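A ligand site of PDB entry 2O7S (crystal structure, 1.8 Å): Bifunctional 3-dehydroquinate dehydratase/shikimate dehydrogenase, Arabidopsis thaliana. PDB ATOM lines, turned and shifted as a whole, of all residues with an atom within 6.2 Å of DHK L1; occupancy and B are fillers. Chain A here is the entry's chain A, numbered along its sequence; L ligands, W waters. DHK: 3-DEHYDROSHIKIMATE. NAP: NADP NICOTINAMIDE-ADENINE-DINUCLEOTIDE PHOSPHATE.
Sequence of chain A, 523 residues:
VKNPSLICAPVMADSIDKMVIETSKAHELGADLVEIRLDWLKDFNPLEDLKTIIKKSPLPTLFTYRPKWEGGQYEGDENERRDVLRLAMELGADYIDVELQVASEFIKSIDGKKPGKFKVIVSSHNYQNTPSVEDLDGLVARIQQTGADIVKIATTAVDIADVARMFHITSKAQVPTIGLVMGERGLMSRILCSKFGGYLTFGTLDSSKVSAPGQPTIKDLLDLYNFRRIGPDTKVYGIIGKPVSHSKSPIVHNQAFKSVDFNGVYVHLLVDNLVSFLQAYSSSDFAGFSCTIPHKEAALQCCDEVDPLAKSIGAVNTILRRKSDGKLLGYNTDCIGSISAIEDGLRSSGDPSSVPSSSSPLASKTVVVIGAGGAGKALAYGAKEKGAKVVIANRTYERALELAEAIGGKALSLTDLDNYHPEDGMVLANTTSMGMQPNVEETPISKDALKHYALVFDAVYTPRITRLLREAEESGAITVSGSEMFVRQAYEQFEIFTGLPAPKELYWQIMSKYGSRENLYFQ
Water W1 lies within hydrogen-bond range of O2 of DHK L1 (2.7 Å), OG1 of Thr 292 (2.8 Å), NE2 of His 246 (2.8 Å) and O2D of NAP L2 (2.9 Å).
The backbone NH (N) of Ser 249 sits at hydrogen-bond distance from the side-chain hydroxyl (OG) of Ser 247, at 3.0 Å.
OD2 of Asp 334 is in salt-bridge range of NZ of Lys 296, at 2.8 Å.
NE2 of Gln 489 sits at hydrogen-bond distance from O of Phe 486 (3.1 Å).
The backbone carbonyl oxygen of Gln 489 lies within hydrogen-bond range of the side-chain hydroxyl of Thr 333 (3.1 Å).
NE2 of Gln 493 sits at hydrogen-bond distance from O of Asn 317 (2.9 Å).
The side-chain amide nitrogen (NE2) of Gln 493 is in hydrogen-bond range of the side-chain hydroxyl (OG1) of Thr 318 (2.9 Å).
The side-chain amide oxygen of Asn 317 sits at hydrogen-bond distance from the side-chain hydroxyl of Thr 333, 2.9 Å away.
OG of Ser 290 sits at hydrogen-bond distance from OH of Tyr 266.
CD1 of Ile 239 touches O1 of DHK L1 (3.6 Å).
CB of Ser 290 touches O5 of DHK L1 (3.6 Å).
O of Cys 291 touches O3 of DHK L1, 3.8 Å away.
Phe 486 touches DHK L1 (CE1 to O1, 3.8 Å).
Within 4 Å of DHK L1: Ile 239, Ser 247, Ser 249, Ser 290, Cys 291, Thr 292, Lys 296, Asn 317, Asp 334, Tyr 461, Phe 486, Gln 489 and Gln 493.
An oxygen (O1) of DHK L1 sits at hydrogen-bond distance from the side-chain hydroxyl (OG) of Ser 247, 2.5 Å away.
The side-chain hydroxyl of Ser 249 lies within hydrogen-bond range of an oxygen (O1) of DHK L1 (2.6 Å).
O2 of DHK L1 sits at hydrogen-bond distance from OH of Tyr 461, at 2.7 Å.
O4 of DHK L1 sits at hydrogen-bond distance from NZ of Lys 296 (2.7 Å).
The side-chain carboxylate of Asp 334 is in hydrogen-bond range of an oxygen (O4) of DHK L1.
O3 of DHK L1 lies within hydrogen-bond range of OG1 of Thr 292.
O5 of DHK L1 is in hydrogen-bond range of OE1 of Gln 489 (2.9 Å).
O5 of DHK L1 sits at hydrogen-bond distance from NE2 of Gln 493 (3.0 Å).
The side-chain amide oxygen of Asn 317 sits at hydrogen-bond distance from an oxygen (O4) of DHK L1 (3.1 Å).
An oxygen (O7N) of NAP L2 lies within hydrogen-bond range of the backbone NH (N) of Phe 486 (3.3 Å).
The backbone NH (N) of Ile 293 lies within hydrogen-bond range of an oxygen (O1N) of NAP L2.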
ATOM      1  N   ILE A 239      24.654 -11.871 -28.823  1.00  0.00           N
ATOM      2  CA  ILE A 239      23.845 -10.682 -28.987  1.00  0.00           C
ATOM      3  C   ILE A 239      24.645  -9.639 -29.782  1.00  0.00           C
ATOM      4  O   ILE A 239      25.703  -9.177 -29.340  1.00  0.00           O
ATOM      5  CB  ILE A 239      23.429 -10.089 -27.607  1.00  0.00           C
ATOM      6  CG1 ILE A 239      22.811  -8.701 -27.799  1.00  0.00           C
ATOM      7  CG2 ILE A 239      24.624 -10.042 -26.649  1.00  0.00           C
ATOM      8  CD1 ILE A 239      21.508  -8.696 -28.603  1.00  0.00           C
ATOM      9  N   HIS A 246      25.550  -3.581 -22.099  1.00  0.00           N
ATOM     10  CA  HIS A 246      24.439  -3.576 -21.153  1.00  0.00           C
ATOM     11  C   HIS A 246      23.586  -4.838 -21.260  1.00  0.00           C
ATOM     12  O   HIS A 246      22.769  -5.105 -20.393  1.00  0.00           O
ATOM     13  CB  HIS A 246      23.534  -2.393 -21.426  1.00  0.00           C
ATOM     14  CG  HIS A 246      22.898  -2.449 -22.782  1.00  0.00           C
ATOM     15  ND1 HIS A 246      23.552  -2.067 -23.927  1.00  0.00           N
ATOM     16  CD2 HIS A 246      21.700  -2.939 -23.181  1.00  0.00           C
ATOM     17  CE1 HIS A 246      22.789  -2.316 -24.974  1.00  0.00           C
ATOM     18  NE2 HIS A 246      21.656  -2.848 -24.550  1.00  0.00           N
ATOM     19  N   SER A 247      23.766  -5.590 -22.342  1.00  0.00           N
ATOM     20  CA  SER A 247      22.918  -6.775 -22.569  1.00  0.00           C
ATOM     21  C   SER A 247      22.988  -7.895 -21.545  1.00  0.00           C
ATOM     22  O   SER A 247      24.062  -8.333 -21.145  1.00  0.00           O
ATOM     23  CB  SER A 247      23.192  -7.371 -23.943  1.00  0.00           C
ATOM     24  OG  SER A 247      22.450  -8.577 -24.105  1.00  0.00           O
ATOM     25  N   LYS A 248      21.804  -8.390 -21.158  1.00  0.00           N
ATOM     26  CA  LYS A 248      21.701  -9.503 -20.226  1.00  0.00           C
ATOM     27  C   LYS A 248      21.338 -10.794 -20.956  1.00  0.00           C
ATOM     28  O   LYS A 248      21.040 -11.798 -20.315  1.00  0.00           O
ATOM     29  CB  LYS A 248      20.652  -9.179 -19.144  1.00  0.00           C
ATOM     30  CG  LYS A 248      21.122  -8.093 -18.189  1.00  0.00           C
ATOM     31  CD  LYS A 248      20.160  -7.867 -17.051  1.00  0.00           C
ATOM     32  CE  LYS A 248      20.747  -6.866 -16.054  1.00  0.00           C
ATOM     33  NZ  LYS A 248      19.760  -6.492 -15.002  1.00  0.00           N
ATOM     34  N   SER A 249      21.351 -10.769 -22.295  1.00  0.00           N
ATOM     35  CA  SER A 249      21.042 -11.987 -23.055  1.00  0.00           C
ATOM     36  C   SER A 249      22.015 -13.105 -22.693  1.00  0.00           C
ATOM     37  O   SER A 249      21.619 -14.267 -22.556  1.00  0.00           O
ATOM     38  CB  SER A 249      21.051 -11.717 -24.569  1.00  0.00           C
ATOM     39  OG  SER A 249      19.804 -11.169 -24.992  1.00  0.00           O
ATOM     40  N   PRO A 250      23.307 -12.779 -22.532  1.00  0.00           N
ATOM     41  CA  PRO A 250      24.244 -13.845 -22.183  1.00  0.00           C
ATOM     42  C   PRO A 250      23.926 -14.464 -20.812  1.00  0.00           C
ATOM     43  O   PRO A 250      24.198 -15.647 -20.574  1.00  0.00           O
ATOM     44  CB  PRO A 250      25.597 -13.142 -22.207  1.00  0.00           C
ATOM     45  CG  PRO A 250      25.396 -12.070 -23.259  1.00  0.00           C
ATOM     46  CD  PRO A 250      24.028 -11.543 -22.908  1.00  0.00           C
ATOM     47  N   TYR A 266      26.698 -18.572 -25.195  1.00  0.00           N
ATOM     48  CA  TYR A 266      26.203 -17.285 -25.693  1.00  0.00           C
ATOM     49  C   TYR A 266      27.091 -16.111 -25.217  1.00  0.00           C
ATOM     50  O   TYR A 266      27.323 -15.971 -24.014  1.00  0.00           O
ATOM     51  CB  TYR A 266      24.760 -17.121 -25.211  1.00  0.00           C
ATOM     52  CG  TYR A 266      23.955 -16.047 -25.899  1.00  0.00           C
ATOM     53  CD1 TYR A 266      24.161 -14.702 -25.602  1.00  0.00           C
ATOM     54  CD2 TYR A 266      22.945 -16.385 -26.820  1.00  0.00           C
ATOM     55  CE1 TYR A 266      23.389 -13.713 -26.197  1.00  0.00           C
ATOM     56  CE2 TYR A 266      22.172 -15.396 -27.415  1.00  0.00           C
ATOM     57  CZ  TYR A 266      22.399 -14.065 -27.101  1.00  0.00           C
ATOM     58  OH  TYR A 266      21.632 -13.072 -27.652  1.00  0.00           O
ATOM     59  N   SER A 290      21.118 -12.873 -31.748  1.00  0.00           N
ATOM     60  CA  SER A 290      20.038 -12.003 -31.342  1.00  0.00           C
ATOM     61  C   SER A 290      20.565 -10.646 -31.839  1.00  0.00           C
ATOM     62  O   SER A 290      21.773 -10.429 -31.857  1.00  0.00           O
ATOM     63  CB  SER A 290      19.891 -11.987 -29.812  1.00  0.00           C
ATOM     64  OG  SER A 290      19.573 -13.275 -29.326  1.00  0.00           O
ATOM     65  N   CYS A 291      19.660  -9.766 -32.258  1.00  0.00           N
ATOM     66  CA  CYS A 291      20.070  -8.451 -32.754  1.00  0.00           C
ATOM     67  C   CYS A 291      19.359  -7.318 -32.056  1.00  0.00           C
ATOM     68  O   CYS A 291      18.133  -7.285 -31.999  1.00  0.00           O
ATOM     69  CB  CYS A 291      19.790  -8.341 -34.257  1.00  0.00           C
ATOM     70  SG  CYS A 291      20.649  -9.533 -35.267  1.00  0.00           S
ATOM     71  N   THR A 292      20.125  -6.364 -31.541  1.00  0.00           N
ATOM     72  CA  THR A 292      19.552  -5.229 -30.871  1.00  0.00           C
ATOM     73  C   THR A 292      20.074  -3.949 -31.510  1.00  0.00           C
ATOM     74  O   THR A 292      20.766  -3.996 -32.528  1.00  0.00           O
ATOM     75  CB  THR A 292      19.878  -5.234 -29.347  1.00  0.00           C
ATOM     76  OG1 THR A 292      19.097  -4.229 -28.688  1.00  0.00           O
ATOM     77  CG2 THR A 292      21.356  -4.968 -29.100  1.00  0.00           C
ATOM     78  N   ILE A 293      19.725  -2.813 -30.919  1.00  0.00           N
ATOM     79  CA  ILE A 293      20.135  -1.507 -31.410  1.00  0.00           C
ATOM     80  C   ILE A 293      21.584  -1.531 -31.895  1.00  0.00           C
ATOM     81  O   ILE A 293      22.479  -1.993 -31.185  1.00  0.00           O
ATOM     82  CB  ILE A 293      19.964  -0.452 -30.278  1.00  0.00           C
ATOM     83  CG1 ILE A 293      20.403   0.920 -30.756  1.00  0.00           C
ATOM     84  CG2 ILE A 293      20.743  -0.892 -29.047  1.00  0.00           C
ATOM     85  CD1 ILE A 293      20.152   2.020 -29.744  1.00  0.00           C
ATOM     86  N   LYS A 296      18.780  -4.016 -36.115  1.00  0.00           N
ATOM     87  CA  LYS A 296      17.563  -4.762 -36.436  1.00  0.00           C
ATOM     88  C   LYS A 296      17.135  -4.647 -37.901  1.00  0.00           C
ATOM     89  O   LYS A 296      16.643  -5.608 -38.488  1.00  0.00           O
ATOM     90  CB  LYS A 296      16.405  -4.326 -35.520  1.00  0.00           C
ATOM     91  CG  LYS A 296      16.576  -4.750 -34.054  1.00  0.00           C
ATOM     92  CD  LYS A 296      15.355  -4.338 -33.219  1.00  0.00           C
ATOM     93  CE  LYS A 296      15.566  -4.597 -31.731  1.00  0.00           C
ATOM     94  NZ  LYS A 296      15.692  -6.042 -31.375  1.00  0.00           N
ATOM     95  N   ASN A 317      15.193  -9.437 -35.220  1.00  0.00           N
ATOM     96  CA  ASN A 317      15.958  -9.468 -33.977  1.00  0.00           C
ATOM     97  C   ASN A 317      16.515 -10.868 -33.695  1.00  0.00           C
ATOM     98  O   ASN A 317      17.193 -11.067 -32.689  1.00  0.00           O
ATOM     99  CB  ASN A 317      15.109  -9.013 -32.787  1.00  0.00           C
ATOM    100  CG  ASN A 317      14.211 -10.108 -32.251  1.00  0.00           C
ATOM    101  OD1 ASN A 317      13.915 -10.150 -31.050  1.00  0.00           O
ATOM    102  ND2 ASN A 317      13.762 -10.995 -33.130  1.00  0.00           N
ATOM    103  N   THR A 318      16.232 -11.821 -34.577  1.00  0.00           N
ATOM    104  CA  THR A 318      16.719 -13.188 -34.397  1.00  0.00           C
ATOM    105  C   THR A 318      17.201 -13.795 -35.720  1.00  0.00           C
ATOM    106  O   THR A 318      16.446 -13.862 -36.703  1.00  0.00           O
ATOM    107  CB  THR A 318      15.623 -14.122 -33.803  1.00  0.00           C
ATOM    108  OG1 THR A 318      14.881 -13.413 -32.803  1.00  0.00           O
ATOM    109  CG2 THR A 318      16.253 -15.342 -33.170  1.00  0.00           C
ATOM    110  N   THR A 333      10.956 -11.697 -32.641  1.00  0.00           N
ATOM    111  CA  THR A 333      10.267 -12.044 -31.403  1.00  0.00           C
ATOM    112  C   THR A 333       9.907 -10.815 -30.570  1.00  0.00           C
ATOM    113  O   THR A 333       9.292 -10.934 -29.511  1.00  0.00           O
ATOM    114  CB  THR A 333      11.125 -13.019 -30.536  1.00  0.00           C
ATOM    115  OG1 THR A 333      12.330 -12.372 -30.128  1.00  0.00           O
ATOM    116  CG2 THR A 333      11.477 -14.270 -31.330  1.00  0.00           C
ATOM    117  N   ASP A 334      10.284  -9.631 -31.051  1.00  0.00           N
ATOM    118  CA  ASP A 334       9.970  -8.384 -30.356  1.00  0.00           C
ATOM    119  C   ASP A 334       8.477  -8.071 -30.337  1.00  0.00           C
ATOM    120  O   ASP A 334       7.941  -7.612 -29.329  1.00  0.00           O
ATOM    121  CB  ASP A 334      10.705  -7.193 -30.992  1.00  0.00           C
ATOM    122  CG  ASP A 334      12.183  -7.134 -30.643  1.00  0.00           C
ATOM    123  OD1 ASP A 334      12.541  -7.378 -29.464  1.00  0.00           O
ATOM    124  OD2 ASP A 334      13.003  -6.819 -31.528  1.00  0.00           O
ATOM    125  N   TYR A 461      15.256  -1.981 -20.788  1.00  0.00           N
ATOM    126  CA  TYR A 461      15.222  -2.837 -19.611  1.00  0.00           C
ATOM    127  C   TYR A 461      16.475  -2.726 -18.738  1.00  0.00           C
ATOM    128  O   TYR A 461      16.609  -3.427 -17.736  1.00  0.00           O
ATOM    129  CB  TYR A 461      14.970  -4.309 -20.000  1.00  0.00           C
ATOM    130  CG  TYR A 461      16.141  -5.012 -20.645  1.00  0.00           C
ATOM    131  CD1 TYR A 461      16.495  -4.767 -21.970  1.00  0.00           C
ATOM    132  CD2 TYR A 461      16.920  -5.916 -19.913  1.00  0.00           C
ATOM    133  CE1 TYR A 461      17.589  -5.399 -22.561  1.00  0.00           C
ATOM    134  CE2 TYR A 461      18.005  -6.559 -20.484  1.00  0.00           C
ATOM    135  CZ  TYR A 461      18.342  -6.293 -21.796  1.00  0.00           C
ATOM    136  OH  TYR A 461      19.433  -6.920 -22.342  1.00  0.00           O
ATOM    137  N   MET A 485       9.038  -7.530 -21.422  1.00  0.00           N
ATOM    138  CA  MET A 485       9.197  -7.731 -22.851  1.00  0.00           C
ATOM    139  C   MET A 485      10.461  -8.544 -23.137  1.00  0.00           C
ATOM    140  O   MET A 485      10.491  -9.382 -24.042  1.00  0.00           O
ATOM    141  CB  MET A 485       9.302  -6.376 -23.565  1.00  0.00           C
ATOM    142  CG  MET A 485       9.668  -6.503 -25.032  1.00  0.00           C
ATOM    143  SD  MET A 485      10.003  -4.903 -25.833  1.00  0.00           S
ATOM    144  CE  MET A 485      10.090  -5.421 -27.565  1.00  0.00           C
ATOM    145  N   PHE A 486      11.515  -8.297 -22.359  1.00  0.00           N
ATOM    146  CA  PHE A 486      12.785  -8.991 -22.528  1.00  0.00           C
ATOM    147  C   PHE A 486      12.706 -10.496 -22.299  1.00  0.00           C
ATOM    148  O   PHE A 486      13.211 -11.276 -23.104  1.00  0.00           O
ATOM    149  CB  PHE A 486      13.845  -8.408 -21.590  1.00  0.00           C
ATOM    150  CG  PHE A 486      15.195  -9.053 -21.733  1.00  0.00           C
ATOM    151  CD1 PHE A 486      15.967  -8.808 -22.864  1.00  0.00           C
ATOM    152  CD2 PHE A 486      15.681  -9.919 -20.768  1.00  0.00           C
ATOM    153  CE1 PHE A 486      17.214  -9.441 -23.032  1.00  0.00           C
ATOM    154  CE2 PHE A 486      16.921 -10.549 -20.912  1.00  0.00           C
ATOM    155  CZ  PHE A 486      17.692 -10.300 -22.056  1.00  0.00           C
ATOM    156  N   GLN A 489      10.540 -12.154 -25.269  1.00  0.00           N
ATOM    157  CA  GLN A 489      11.190 -12.295 -26.555  1.00  0.00           C
ATOM    158  C   GLN A 489      12.361 -13.264 -26.453  1.00  0.00           C
ATOM    159  O   GLN A 489      12.727 -13.908 -27.446  1.00  0.00           O
ATOM    160  CB  GLN A 489      11.675 -10.927 -27.075  1.00  0.00           C
ATOM    161  CG  GLN A 489      12.787 -10.277 -26.271  1.00  0.00           C
ATOM    162  CD  GLN A 489      14.165 -10.813 -26.617  1.00  0.00           C
ATOM    163  OE1 GLN A 489      14.458 -11.102 -27.781  1.00  0.00           O
ATOM    164  NE2 GLN A 489      15.023 -10.927 -25.615  1.00  0.00           N
ATOM    165  N   GLN A 493      13.304 -16.918 -28.532  1.00  0.00           N
ATOM    166  CA  GLN A 493      14.556 -17.070 -29.270  1.00  0.00           C
ATOM    167  C   GLN A 493      15.221 -18.401 -28.908  1.00  0.00           C
ATOM    168  O   GLN A 493      15.882 -19.019 -29.747  1.00  0.00           O
ATOM    169  CB  GLN A 493      15.532 -15.913 -28.967  1.00  0.00           C
ATOM    170  CG  GLN A 493      15.133 -14.541 -29.512  1.00  0.00           C
ATOM    171  CD  GLN A 493      16.275 -13.534 -29.457  1.00  0.00           C
ATOM    172  OE1 GLN A 493      17.077 -13.535 -28.525  1.00  0.00           O
ATOM    173  NE2 GLN A 493      16.342 -12.655 -30.464  1.00  0.00           N
HETATM  174  C2  DHK L   1      17.561  -6.592 -26.724  1.00  0.00           C
HETATM  175  C3  DHK L   1      16.391  -6.592 -27.680  1.00  0.00           C
HETATM  176  O3  DHK L   1      16.717  -5.741 -28.791  1.00  0.00           O
HETATM  177  C4  DHK L   1      16.018  -8.007 -28.212  1.00  0.00           C
HETATM  178  O4  DHK L   1      15.257  -7.883 -29.418  1.00  0.00           O
HETATM  179  C5  DHK L   1      17.292  -8.854 -28.456  1.00  0.00           C
HETATM  180  C1  DHK L   1      18.315  -7.645 -26.479  1.00  0.00           C
HETATM  181  C6  DHK L   1      18.103  -9.000 -27.150  1.00  0.00           C
HETATM  182  C   DHK L   1      19.428  -7.513 -25.522  1.00  0.00           C
HETATM  183  O1  DHK L   1      20.203  -8.572 -25.266  1.00  0.00           O
HETATM  184  O2  DHK L   1      19.646  -6.441 -24.963  1.00  0.00           O
HETATM  185  O5  DHK L   1      16.936 -10.157 -28.940  1.00  0.00           O
HETATM  186  PA  NAP L   2      16.876   1.618 -33.243  1.00  0.00           P
HETATM  187  O1A NAP L   2      18.316   1.955 -33.129  1.00  0.00           O
HETATM  188  O2A NAP L   2      16.430   0.323 -33.812  1.00  0.00           O
HETATM  189  O5B NAP L   2      15.800   2.432 -32.339  1.00  0.00           O
HETATM  190  C5B NAP L   2      16.416   3.586 -31.740  1.00  0.00           C
HETATM  191  C4B NAP L   2      15.419   4.723 -31.562  1.00  0.00           C
HETATM  192  O4B NAP L   2      16.026   5.567 -30.591  1.00  0.00           O
HETATM  193  C3B NAP L   2      14.944   5.745 -32.579  1.00  0.00           C
HETATM  194  O3B NAP L   2      13.524   5.976 -32.630  1.00  0.00           O
HETATM  195  C2B NAP L   2      16.127   6.738 -32.677  1.00  0.00           C
HETATM  196  O2B NAP L   2      15.689   8.108 -32.869  1.00  0.00           O
HETATM  197  C1B NAP L   2      16.795   6.496 -31.287  1.00  0.00           C
HETATM  198  N9A NAP L   2      17.227   7.589 -30.400  1.00  0.00           N
HETATM  199  C8A NAP L   2      18.515   7.740 -29.857  1.00  0.00           C
HETATM  200  N7A NAP L   2      18.561   8.851 -29.075  1.00  0.00           N
HETATM  201  C5A NAP L   2      17.303   9.371 -29.145  1.00  0.00           C
HETATM  202  C6A NAP L   2      16.840  10.519 -28.504  1.00  0.00           C
HETATM  203  N6A NAP L   2      17.670  11.225 -27.740  1.00  0.00           N
HETATM  204  N1A NAP L   2      15.507  10.932 -28.673  1.00  0.00           N
HETATM  205  C2A NAP L   2      14.669  10.134 -29.510  1.00  0.00           C
HETATM  206  N3A NAP L   2      15.184   8.974 -30.129  1.00  0.00           N
HETATM  207  C4A NAP L   2      16.527   8.666 -29.885  1.00  0.00           C
HETATM  208  O3  NAP L   2      17.220   0.839 -31.863  1.00  0.00           O
HETATM  209  PN  NAP L   2      16.209  -0.407 -31.367  1.00  0.00           P
HETATM  210  O1N NAP L   2      16.684  -1.675 -31.972  1.00  0.00           O
HETATM  211  O2N NAP L   2      14.786  -0.163 -31.795  1.00  0.00           O
HETATM  212  O5D NAP L   2      16.276  -0.558 -29.752  1.00  0.00           O
HETATM  213  C5D NAP L   2      15.813   0.648 -29.075  1.00  0.00           C
HETATM  214  C4D NAP L   2      15.835   0.527 -27.528  1.00  0.00           C
HETATM  215  O4D NAP L   2      14.741  -0.270 -26.960  1.00  0.00           O
HETATM  216  C3D NAP L   2      17.156  -0.067 -26.948  1.00  0.00           C
HETATM  217  O3D NAP L   2      17.537   0.757 -25.815  1.00  0.00           O
HETATM  218  C2D NAP L   2      16.824  -1.431 -26.508  1.00  0.00           C
HETATM  219  O2D NAP L   2      17.529  -1.821 -25.353  1.00  0.00           O
HETATM  220  C1D NAP L   2      15.303  -1.419 -26.274  1.00  0.00           C
HETATM  221  N1N NAP L   2      14.661  -2.704 -26.633  1.00  0.00           N
HETATM  222  C2N NAP L   2      14.325  -3.535 -25.545  1.00  0.00           C
HETATM  223  C3N NAP L   2      13.700  -4.767 -25.892  1.00  0.00           C
HETATM  224  C7N NAP L   2      13.311  -5.705 -24.810  1.00  0.00           C
HETATM  225  O7N NAP L   2      12.765  -6.778 -25.069  1.00  0.00           O
HETATM  226  N7N NAP L   2      13.553  -5.381 -23.521  1.00  0.00           N
HETATM  227  C4N NAP L   2      13.424  -5.118 -27.265  1.00  0.00           C
HETATM  228  C5N NAP L   2      13.781  -4.253 -28.296  1.00  0.00           C
HETATM  229  C6N NAP L   2      14.409  -3.022 -28.007  1.00  0.00           C
HETATM  230  P2B NAP L   2      15.819   8.511 -34.427  1.00  0.00           P
HETATM  231  O1X NAP L   2      14.921   7.633 -35.263  1.00  0.00           O
HETATM  232  O2X NAP L   2      15.392   9.877 -34.606  1.00  0.00           O
HETATM  233  O3X NAP L   2      17.206   8.347 -34.875  1.00  0.00           O
HETATM  234  O   HOH W   1      19.451  -3.935 -25.948  1.00  0.00           O
